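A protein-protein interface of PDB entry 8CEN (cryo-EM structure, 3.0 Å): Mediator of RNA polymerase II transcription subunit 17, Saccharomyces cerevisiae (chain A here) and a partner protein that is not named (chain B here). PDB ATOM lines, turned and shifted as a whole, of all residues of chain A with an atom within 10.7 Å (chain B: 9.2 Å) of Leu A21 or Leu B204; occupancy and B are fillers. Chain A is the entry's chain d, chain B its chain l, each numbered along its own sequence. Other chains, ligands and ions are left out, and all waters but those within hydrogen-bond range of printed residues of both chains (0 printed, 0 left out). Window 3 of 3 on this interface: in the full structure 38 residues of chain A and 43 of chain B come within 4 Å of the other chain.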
ATOM      1  N   ILE A  17       6.280   9.395 -24.867  1.00  0.00           N
ATOM      2  CA  ILE A  17       7.160   9.445 -26.027  1.00  0.00           C
ATOM      3  C   ILE A  17       7.856  10.802 -26.042  1.00  0.00           C
ATOM      4  O   ILE A  17       7.302  11.812 -25.599  1.00  0.00           O
ATOM      5  CB  ILE A  17       6.381   9.167 -27.343  1.00  0.00           C
ATOM      6  CG1 ILE A  17       7.335   8.962 -28.526  1.00  0.00           C
ATOM      7  CG2 ILE A  17       5.359  10.264 -27.636  1.00  0.00           C
ATOM      8  CD1 ILE A  17       6.676   8.376 -29.750  1.00  0.00           C
ATOM      9  N   LYS A  18       9.098  10.812 -26.522  1.00  0.00           N
ATOM     10  CA  LYS A  18       9.873  12.039 -26.603  1.00  0.00           C
ATOM     11  C   LYS A  18       9.311  12.953 -27.692  1.00  0.00           C
ATOM     12  O   LYS A  18       8.480  12.555 -28.511  1.00  0.00           O
ATOM     13  CB  LYS A  18      11.339  11.721 -26.882  1.00  0.00           C
ATOM     14  CG  LYS A  18      11.951  10.704 -25.936  1.00  0.00           C
ATOM     15  CD  LYS A  18      13.224  10.114 -26.520  1.00  0.00           C
ATOM     16  CE  LYS A  18      13.764   8.986 -25.656  1.00  0.00           C
ATOM     17  NZ  LYS A  18      14.890   8.273 -26.322  1.00  0.00           N
ATOM     18  N   LEU A  19       9.773  14.202 -27.689  1.00  0.00           N
ATOM     19  CA  LEU A  19       9.343  15.191 -28.670  1.00  0.00           C
ATOM     20  C   LEU A  19      10.548  15.881 -29.287  1.00  0.00           C
ATOM     21  O   LEU A  19      11.434  16.357 -28.571  1.00  0.00           O
ATOM     22  CB  LEU A  19       8.406  16.228 -28.050  1.00  0.00           C
ATOM     23  CG  LEU A  19       6.919  15.894 -28.093  1.00  0.00           C
ATOM     24  CD1 LEU A  19       6.111  16.974 -27.398  1.00  0.00           C
ATOM     25  CD2 LEU A  19       6.505  15.773 -29.542  1.00  0.00           C
ATOM     26  N   ALA A  20      10.570  15.935 -30.616  1.00  0.00           N
ATOM     27  CA  ALA A  20      11.563  16.693 -31.366  1.00  0.00           C
ATOM     28  C   ALA A  20      10.947  18.030 -31.747  1.00  0.00           C
ATOM     29  O   ALA A  20       9.901  18.071 -32.404  1.00  0.00           O
ATOM     30  CB  ALA A  20      12.016  15.931 -32.610  1.00  0.00           C
ATOM     31  N   LEU A  21      11.589  19.118 -31.332  1.00  0.00           N
ATOM     32  CA  LEU A  21      11.035  20.451 -31.501  1.00  0.00           C
ATOM     33  C   LEU A  21      12.133  21.425 -31.890  1.00  0.00           C
ATOM     34  O   LEU A  21      13.312  21.207 -31.598  1.00  0.00           O
ATOM     35  CB  LEU A  21      10.340  20.926 -30.218  1.00  0.00           C
ATOM     36  CG  LEU A  21       8.828  20.718 -30.189  1.00  0.00           C
ATOM     37  CD1 LEU A  21       8.241  21.193 -28.887  1.00  0.00           C
ATOM     38  CD2 LEU A  21       8.217  21.489 -31.328  1.00  0.00           C
ATOM     39  N   ASP A  22      11.734  22.497 -32.567  1.00  0.00           N
ATOM     40  CA  ASP A  22      12.633  23.606 -32.848  1.00  0.00           C
ATOM     41  C   ASP A  22      12.447  24.658 -31.762  1.00  0.00           C
ATOM     42  O   ASP A  22      11.464  25.408 -31.787  1.00  0.00           O
ATOM     43  CB  ASP A  22      12.360  24.196 -34.232  1.00  0.00           C
ATOM     44  CG  ASP A  22      13.570  24.897 -34.818  1.00  0.00           C
ATOM     45  OD1 ASP A  22      14.481  25.270 -34.049  1.00  0.00           O
ATOM     46  OD2 ASP A  22      13.610  25.078 -36.053  1.00  0.00           O
ATOM     47  N   PRO A  23      13.366  24.745 -30.796  1.00  0.00           N
ATOM     48  CA  PRO A  23      13.162  25.670 -29.671  1.00  0.00           C
ATOM     49  C   PRO A  23      13.390  27.128 -30.023  1.00  0.00           C
ATOM     50  O   PRO A  23      13.052  27.994 -29.207  1.00  0.00           O
ATOM     51  CB  PRO A  23      14.179  25.186 -28.633  1.00  0.00           C
ATOM     52  CG  PRO A  23      15.263  24.566 -29.434  1.00  0.00           C
ATOM     53  CD  PRO A  23      14.671  24.066 -30.726  1.00  0.00           C
ATOM     54  N   ASN A  24      13.944  27.424 -31.202  1.00  0.00           N
ATOM     55  CA  ASN A  24      14.200  28.809 -31.582  1.00  0.00           C
ATOM     56  C   ASN A  24      12.910  29.601 -31.749  1.00  0.00           C
ATOM     57  O   ASN A  24      12.891  30.812 -31.499  1.00  0.00           O
ATOM     58  CB  ASN A  24      15.020  28.855 -32.872  1.00  0.00           C
ATOM     59  CG  ASN A  24      16.369  28.184 -32.726  1.00  0.00           C
ATOM     60  OD1 ASN A  24      17.024  28.306 -31.693  1.00  0.00           O
ATOM     61  ND2 ASN A  24      16.788  27.466 -33.761  1.00  0.00           N
ATOM     62  N   LEU A  25      11.831  28.946 -32.167  1.00  0.00           N
ATOM     63  CA  LEU A  25      10.541  29.601 -32.354  1.00  0.00           C
ATOM     64  C   LEU A  25       9.473  28.791 -31.630  1.00  0.00           C
ATOM     65  O   LEU A  25       9.315  27.592 -31.881  1.00  0.00           O
ATOM     66  CB  LEU A  25      10.242  29.788 -33.847  1.00  0.00           C
ATOM     67  CG  LEU A  25      10.095  28.671 -34.891  1.00  0.00           C
ATOM     68  CD1 LEU A  25       8.709  28.029 -34.963  1.00  0.00           C
ATOM     69  CD2 LEU A  25      10.516  29.204 -36.238  1.00  0.00           C
ATOM     70  N   ILE A  26       8.800  29.426 -30.671  1.00  0.00           N
ATOM     71  CA  ILE A  26       7.742  28.781 -29.903  1.00  0.00           C
ATOM     72  C   ILE A  26       6.462  29.592 -30.067  1.00  0.00           C
ATOM     73  O   ILE A  26       5.353  29.051 -30.009  1.00  0.00           O
ATOM     74  CB  ILE A  26       8.128  28.648 -28.416  1.00  0.00           C
ATOM     75  CG1 ILE A  26       9.553  28.107 -28.270  1.00  0.00           C
ATOM     76  CG2 ILE A  26       7.167  27.724 -27.688  1.00  0.00           C
ATOM     77  CD1 ILE A  26       9.715  26.678 -28.722  1.00  0.00           C
ATOM     78  N   THR A  27       6.610  30.893 -30.295  1.00  0.00           N
ATOM     79  CA  THR A  27       5.455  31.775 -30.384  1.00  0.00           C
ATOM     80  C   THR A  27       4.744  31.613 -31.724  1.00  0.00           C
ATOM     81  O   THR A  27       5.369  31.399 -32.766  1.00  0.00           O
ATOM     82  CB  THR A  27       5.876  33.231 -30.191  1.00  0.00           C
ATOM     83  OG1 THR A  27       6.792  33.605 -31.228  1.00  0.00           O
ATOM     84  CG2 THR A  27       6.550  33.415 -28.838  1.00  0.00           C
ATOM     85  N   LEU A  28       3.419  31.719 -31.684  1.00  0.00           N
ATOM     86  CA  LEU A  28       2.605  31.636 -32.884  1.00  0.00           C
ATOM     87  C   LEU A  28       2.608  32.973 -33.624  1.00  0.00           C
ATOM     88  O   LEU A  28       3.032  34.007 -33.100  1.00  0.00           O
ATOM     89  CB  LEU A  28       1.169  31.221 -32.549  1.00  0.00           C
ATOM     90  CG  LEU A  28       0.183  32.195 -31.888  1.00  0.00           C
ATOM     91  CD1 LEU A  28      -1.235  31.669 -32.048  1.00  0.00           C
ATOM     92  CD2 LEU A  28       0.478  32.428 -30.412  1.00  0.00           C
ATOM     93  N   LEU A  86      15.866  31.542 -27.954  1.00  0.00           N
ATOM     94  CA  LEU A  86      16.357  31.069 -26.664  1.00  0.00           C
ATOM     95  C   LEU A  86      17.599  30.198 -26.821  1.00  0.00           C
ATOM     96  O   LEU A  86      18.477  30.215 -25.952  1.00  0.00           O
ATOM     97  CB  LEU A  86      15.236  30.341 -25.915  1.00  0.00           C
ATOM     98  CG  LEU A  86      14.524  29.119 -26.507  1.00  0.00           C
ATOM     99  CD1 LEU A  86      15.209  27.798 -26.184  1.00  0.00           C
ATOM    100  CD2 LEU A  86      13.070  29.089 -26.065  1.00  0.00           C
ATOM    101  N   VAL A  87      17.695  29.439 -27.908  1.00  0.00           N
ATOM    102  CA  VAL A  87      18.935  28.768 -28.276  1.00  0.00           C
ATOM    103  C   VAL A  87      19.705  29.697 -29.204  1.00  0.00           C
ATOM    104  O   VAL A  87      19.202  30.088 -30.263  1.00  0.00           O
ATOM    105  CB  VAL A  87      18.670  27.409 -28.941  1.00  0.00           C
ATOM    106  CG1 VAL A  87      19.935  26.889 -29.605  1.00  0.00           C
ATOM    107  CG2 VAL A  87      18.172  26.407 -27.916  1.00  0.00           C
ATOM    108  N   ASP B 199       0.912  26.381 -20.328  1.00  0.00           N
ATOM    109  CA  ASP B 199       2.088  27.188 -20.667  1.00  0.00           C
ATOM    110  C   ASP B 199       3.160  26.297 -21.292  1.00  0.00           C
ATOM    111  O   ASP B 199       4.165  25.932 -20.664  1.00  0.00           O
ATOM    112  CB  ASP B 199       2.610  27.926 -19.452  1.00  0.00           C
ATOM    113  CG  ASP B 199       3.260  29.242 -19.818  1.00  0.00           C
ATOM    114  OD1 ASP B 199       3.821  29.341 -20.930  1.00  0.00           O
ATOM    115  OD2 ASP B 199       3.196  30.189 -19.011  1.00  0.00           O
ATOM    116  N   LEU B 200       2.981  26.035 -22.587  1.00  0.00           N
ATOM    117  CA  LEU B 200       3.958  25.263 -23.337  1.00  0.00           C
ATOM    118  C   LEU B 200       5.239  26.051 -23.553  1.00  0.00           C
ATOM    119  O   LEU B 200       6.314  25.454 -23.619  1.00  0.00           O
ATOM    120  CB  LEU B 200       3.368  24.831 -24.678  1.00  0.00           C
ATOM    121  CG  LEU B 200       2.048  24.063 -24.612  1.00  0.00           C
ATOM    122  CD1 LEU B 200       1.383  24.051 -25.972  1.00  0.00           C
ATOM    123  CD2 LEU B 200       2.276  22.647 -24.112  1.00  0.00           C
ATOM    124  N   VAL B 201       5.146  27.380 -23.649  1.00  0.00           N
ATOM    125  CA  VAL B 201       6.330  28.204 -23.885  1.00  0.00           C
ATOM    126  C   VAL B 201       7.293  28.098 -22.708  1.00  0.00           C
ATOM    127  O   VAL B 201       8.483  27.792 -22.875  1.00  0.00           O
ATOM    128  CB  VAL B 201       5.917  29.667 -24.137  1.00  0.00           C
ATOM    129  CG1 VAL B 201       7.134  30.577 -24.144  1.00  0.00           C
ATOM    130  CG2 VAL B 201       5.122  29.791 -25.427  1.00  0.00           C
ATOM    131  N   THR B 202       6.777  28.310 -21.495  1.00  0.00           N
ATOM    132  CA  THR B 202       7.608  28.211 -20.302  1.00  0.00           C
ATOM    133  C   THR B 202       8.053  26.776 -20.059  1.00  0.00           C
ATOM    134  O   THR B 202       9.190  26.543 -19.625  1.00  0.00           O
ATOM    135  CB  THR B 202       6.857  28.766 -19.091  1.00  0.00           C
ATOM    136  OG1 THR B 202       6.237  30.007 -19.447  1.00  0.00           O
ATOM    137  CG2 THR B 202       7.816  29.016 -17.936  1.00  0.00           C
ATOM    138  N   ALA B 203       7.183  25.799 -20.358  1.00  0.00           N
ATOM    139  CA  ALA B 203       7.579  24.400 -20.212  1.00  0.00           C
ATOM    140  C   ALA B 203       8.752  24.046 -21.123  1.00  0.00           C
ATOM    141  O   ALA B 203       9.711  23.402 -20.683  1.00  0.00           O
ATOM    142  CB  ALA B 203       6.394  23.484 -20.499  1.00  0.00           C
ATOM    143  N   LEU B 204       8.702  24.477 -22.389  1.00  0.00           N
ATOM    144  CA  LEU B 204       9.808  24.230 -23.311  1.00  0.00           C
ATOM    145  C   LEU B 204      11.080  24.950 -22.896  1.00  0.00           C
ATOM    146  O   LEU B 204      12.164  24.362 -22.972  1.00  0.00           O
ATOM    147  CB  LEU B 204       9.418  24.615 -24.737  1.00  0.00           C
ATOM    148  CG  LEU B 204       8.354  23.715 -25.343  1.00  0.00           C
ATOM    149  CD1 LEU B 204       7.894  24.226 -26.677  1.00  0.00           C
ATOM    150  CD2 LEU B 204       9.027  22.391 -25.524  1.00  0.00           C
ATOM    151  N   GLU B 205      10.977  26.209 -22.453  1.00  0.00           N
ATOM    152  CA  GLU B 205      12.180  26.924 -22.026  1.00  0.00           C
ATOM    153  C   GLU B 205      12.851  26.224 -20.850  1.00  0.00           C
ATOM    154  O   GLU B 205      14.067  25.988 -20.866  1.00  0.00           O
ATOM    155  CB  GLU B 205      11.859  28.376 -21.663  1.00  0.00           C
ATOM    156  CG  GLU B 205      11.367  29.235 -22.809  1.00  0.00           C
ATOM    157  CD  GLU B 205      10.463  30.360 -22.344  1.00  0.00           C
ATOM    158  OE1 GLU B 205       9.994  30.309 -21.190  1.00  0.00           O
ATOM    159  OE2 GLU B 205      10.228  31.301 -23.132  1.00  0.00           O
ATOM    160  N   VAL B 206      12.064  25.835 -19.844  1.00  0.00           N
ATOM    161  CA  VAL B 206      12.643  25.233 -18.647  1.00  0.00           C
ATOM    162  C   VAL B 206      13.162  23.827 -18.936  1.00  0.00           C
ATOM    163  O   VAL B 206      14.245  23.447 -18.478  1.00  0.00           O
ATOM    164  CB  VAL B 206      11.619  25.248 -17.503  1.00  0.00           C
ATOM    165  CG1 VAL B 206      12.170  24.547 -16.284  1.00  0.00           C
ATOM    166  CG2 VAL B 206      11.271  26.668 -17.166  1.00  0.00           C
ATOM    167  N   LEU B 207      12.424  23.035 -19.711  1.00  0.00           N
ATOM    168  CA  LEU B 207      12.881  21.679 -19.972  1.00  0.00           C
ATOM    169  C   LEU B 207      13.942  21.604 -21.062  1.00  0.00           C
ATOM    170  O   LEU B 207      14.526  20.533 -21.257  1.00  0.00           O
ATOM    171  CB  LEU B 207      11.694  20.786 -20.333  1.00  0.00           C
ATOM    172  CG  LEU B 207      10.644  20.572 -19.242  1.00  0.00           C
ATOM    173  CD1 LEU B 207       9.613  19.548 -19.685  1.00  0.00           C
ATOM    174  CD2 LEU B 207      11.300  20.158 -17.940  1.00  0.00           C
ATOM    175  N   SER B 208      14.208  22.700 -21.778  1.00  0.00           N
ATOM    176  CA  SER B 208      15.288  22.738 -22.754  1.00  0.00           C
ATOM    177  C   SER B 208      16.567  23.330 -22.171  1.00  0.00           C
ATOM    178  O   SER B 208      17.604  22.662 -22.137  1.00  0.00           O
ATOM    179  CB  SER B 208      14.847  23.537 -23.986  1.00  0.00           C
ATOM    180  OG  SER B 208      13.768  22.899 -24.646  1.00  0.00           O
ATOM    181  N   LEU B 209      16.514  24.579 -21.709  1.00  0.00           N
ATOM    182  CA  LEU B 209      17.714  25.262 -21.245  1.00  0.00           C
ATOM    183  C   LEU B 209      17.922  25.176 -19.741  1.00  0.00           C
ATOM    184  O   LEU B 209      18.979  25.593 -19.256  1.00  0.00           O
ATOM    185  CB  LEU B 209      17.678  26.739 -21.651  1.00  0.00           C
ATOM    186  CG  LEU B 209      17.298  27.103 -23.083  1.00  0.00           C
ATOM    187  CD1 LEU B 209      17.303  28.614 -23.237  1.00  0.00           C
ATOM    188  CD2 LEU B 209      18.246  26.455 -24.077  1.00  0.00           C
ATOM    189  N   GLY B 210      16.953  24.654 -18.994  1.00  0.00           N
ATOM    190  CA  GLY B 210      16.996  24.751 -17.554  1.00  0.00           C
ATOM    191  C   GLY B 210      16.610  26.104 -17.010  1.00  0.00           C
ATOM    192  O   GLY B 210      16.718  26.324 -15.797  1.00  0.00           O
ATOM    193  N   ARG B 211      16.157  27.014 -17.867  1.00  0.00           N
ATOM    194  CA  ARG B 211      15.862  28.390 -17.510  1.00  0.00           C
ATOM    195  C   ARG B 211      14.725  28.873 -18.394  1.00  0.00           C
ATOM    196  O   ARG B 211      14.619  28.450 -19.552  1.00  0.00           O
ATOM    197  CB  ARG B 211      17.103  29.288 -17.680  1.00  0.00           C
ATOM    198  CG  ARG B 211      17.535  29.458 -19.135  1.00  0.00           C
ATOM    199  CD  ARG B 211      18.817  30.232 -19.358  1.00  0.00           C
ATOM    200  NE  ARG B 211      18.992  30.460 -20.789  1.00  0.00           N
ATOM    201  CZ  ARG B 211      20.079  30.963 -21.356  1.00  0.00           C
ATOM    202  NH1 ARG B 211      21.140  31.299 -20.643  1.00  0.00           N
ATOM    203  NH2 ARG B 211      20.107  31.125 -22.675  1.00  0.00           N
ATOM    204  N   PRO B 212      13.827  29.693 -17.868  1.00  0.00           N
ATOM    205  CA  PRO B 212      12.936  30.456 -18.743  1.00  0.00           C
ATOM    206  C   PRO B 212      13.714  31.549 -19.456  1.00  0.00           C
ATOM    207  O   PRO B 212      14.716  32.060 -18.952  1.00  0.00           O
ATOM    208  CB  PRO B 212      11.894  31.033 -17.781  1.00  0.00           C
ATOM    209  CG  PRO B 212      12.560  31.022 -16.453  1.00  0.00           C
ATOM    210  CD  PRO B 212      13.482  29.849 -16.449  1.00  0.00           C
ATOM    211  N   ASN B 213      13.245  31.901 -20.648  1.00  0.00           N
ATOM    212  CA  ASN B 213      13.969  32.837 -21.503  1.00  0.00           C
ATOM    213  C   ASN B 213      13.670  34.259 -21.044  1.00  0.00           C
ATOM    214  O   ASN B 213      12.612  34.815 -21.344  1.00  0.00           O
ATOM    215  CB  ASN B 213      13.589  32.633 -22.965  1.00  0.00           C
ATOM    216  CG  ASN B 213      14.306  33.592 -23.891  1.00  0.00           C
ATOM    217  OD1 ASN B 213      15.481  33.404 -24.209  1.00  0.00           O
ATOM    218  ND2 ASN B 213      13.603  34.629 -24.329  1.00  0.00           N
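No residue of chain B comes within 4 Å of Ala A20.
Of the printed residues of chain B, Leu A21 touches Leu B204 (3.7 Å).
Leu A25 touches none of the printed residues of chain B.
Leu B200 touches none of the printed residues of chain A.
Of chain A, only Ile A26 (3.7 Å) comes within 4 Å of Val B201.
No residue of chain A comes within 4 Å of Ala B203.
Leu B204 touches two residues of chain A.
Of chain A, only Leu A86 comes within 4 Å of Glu B205.
Val B206 touches none of the printed residues of chain A.
No residue of chain A comes within 4 Å of Leu B207.
No residue of chain A comes within 4 Å of Ser B208.
Of the printed residues of chain A, Arg B211 touches Leu A86.
Printed residues of chain A within 4 Å of Asn B213: Leu A86.
The nearest printed residue of chain A that does not touch Leu B209 is Pro A23 (6.2 Å).
Among the printed residues, pairs that only touch across the chains: Leu A86 with Leu B209, Leu A86 with Asn B213, Leu A21 with Leu B204, Ile A26 with Leu B204, Leu A86 with Glu B205, Ile A26 with Val B201, Leu A86 with Arg B211 and Val A87 with Leu B209.
OD1 of Asn A24 sits close to O of Val A87 (3.2 Å).
The backbone carbonyl oxygen (O) of Leu B204 is in hydrogen-bond range of the side-chain hydroxyl (OG) of Ser B208 (2.7 Å).
Hydrophobic or aromatic side chains of chain B that line the printed part of chain A: Val B201, Leu B204 and Leu B209.
Hydrophobic or aromatic side chains of chain A that line the printed part of chain B: Leu A21, Ile A26, Leu A86 and Val A87.
Among the printed residues, 8 pairs touch across the chains.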
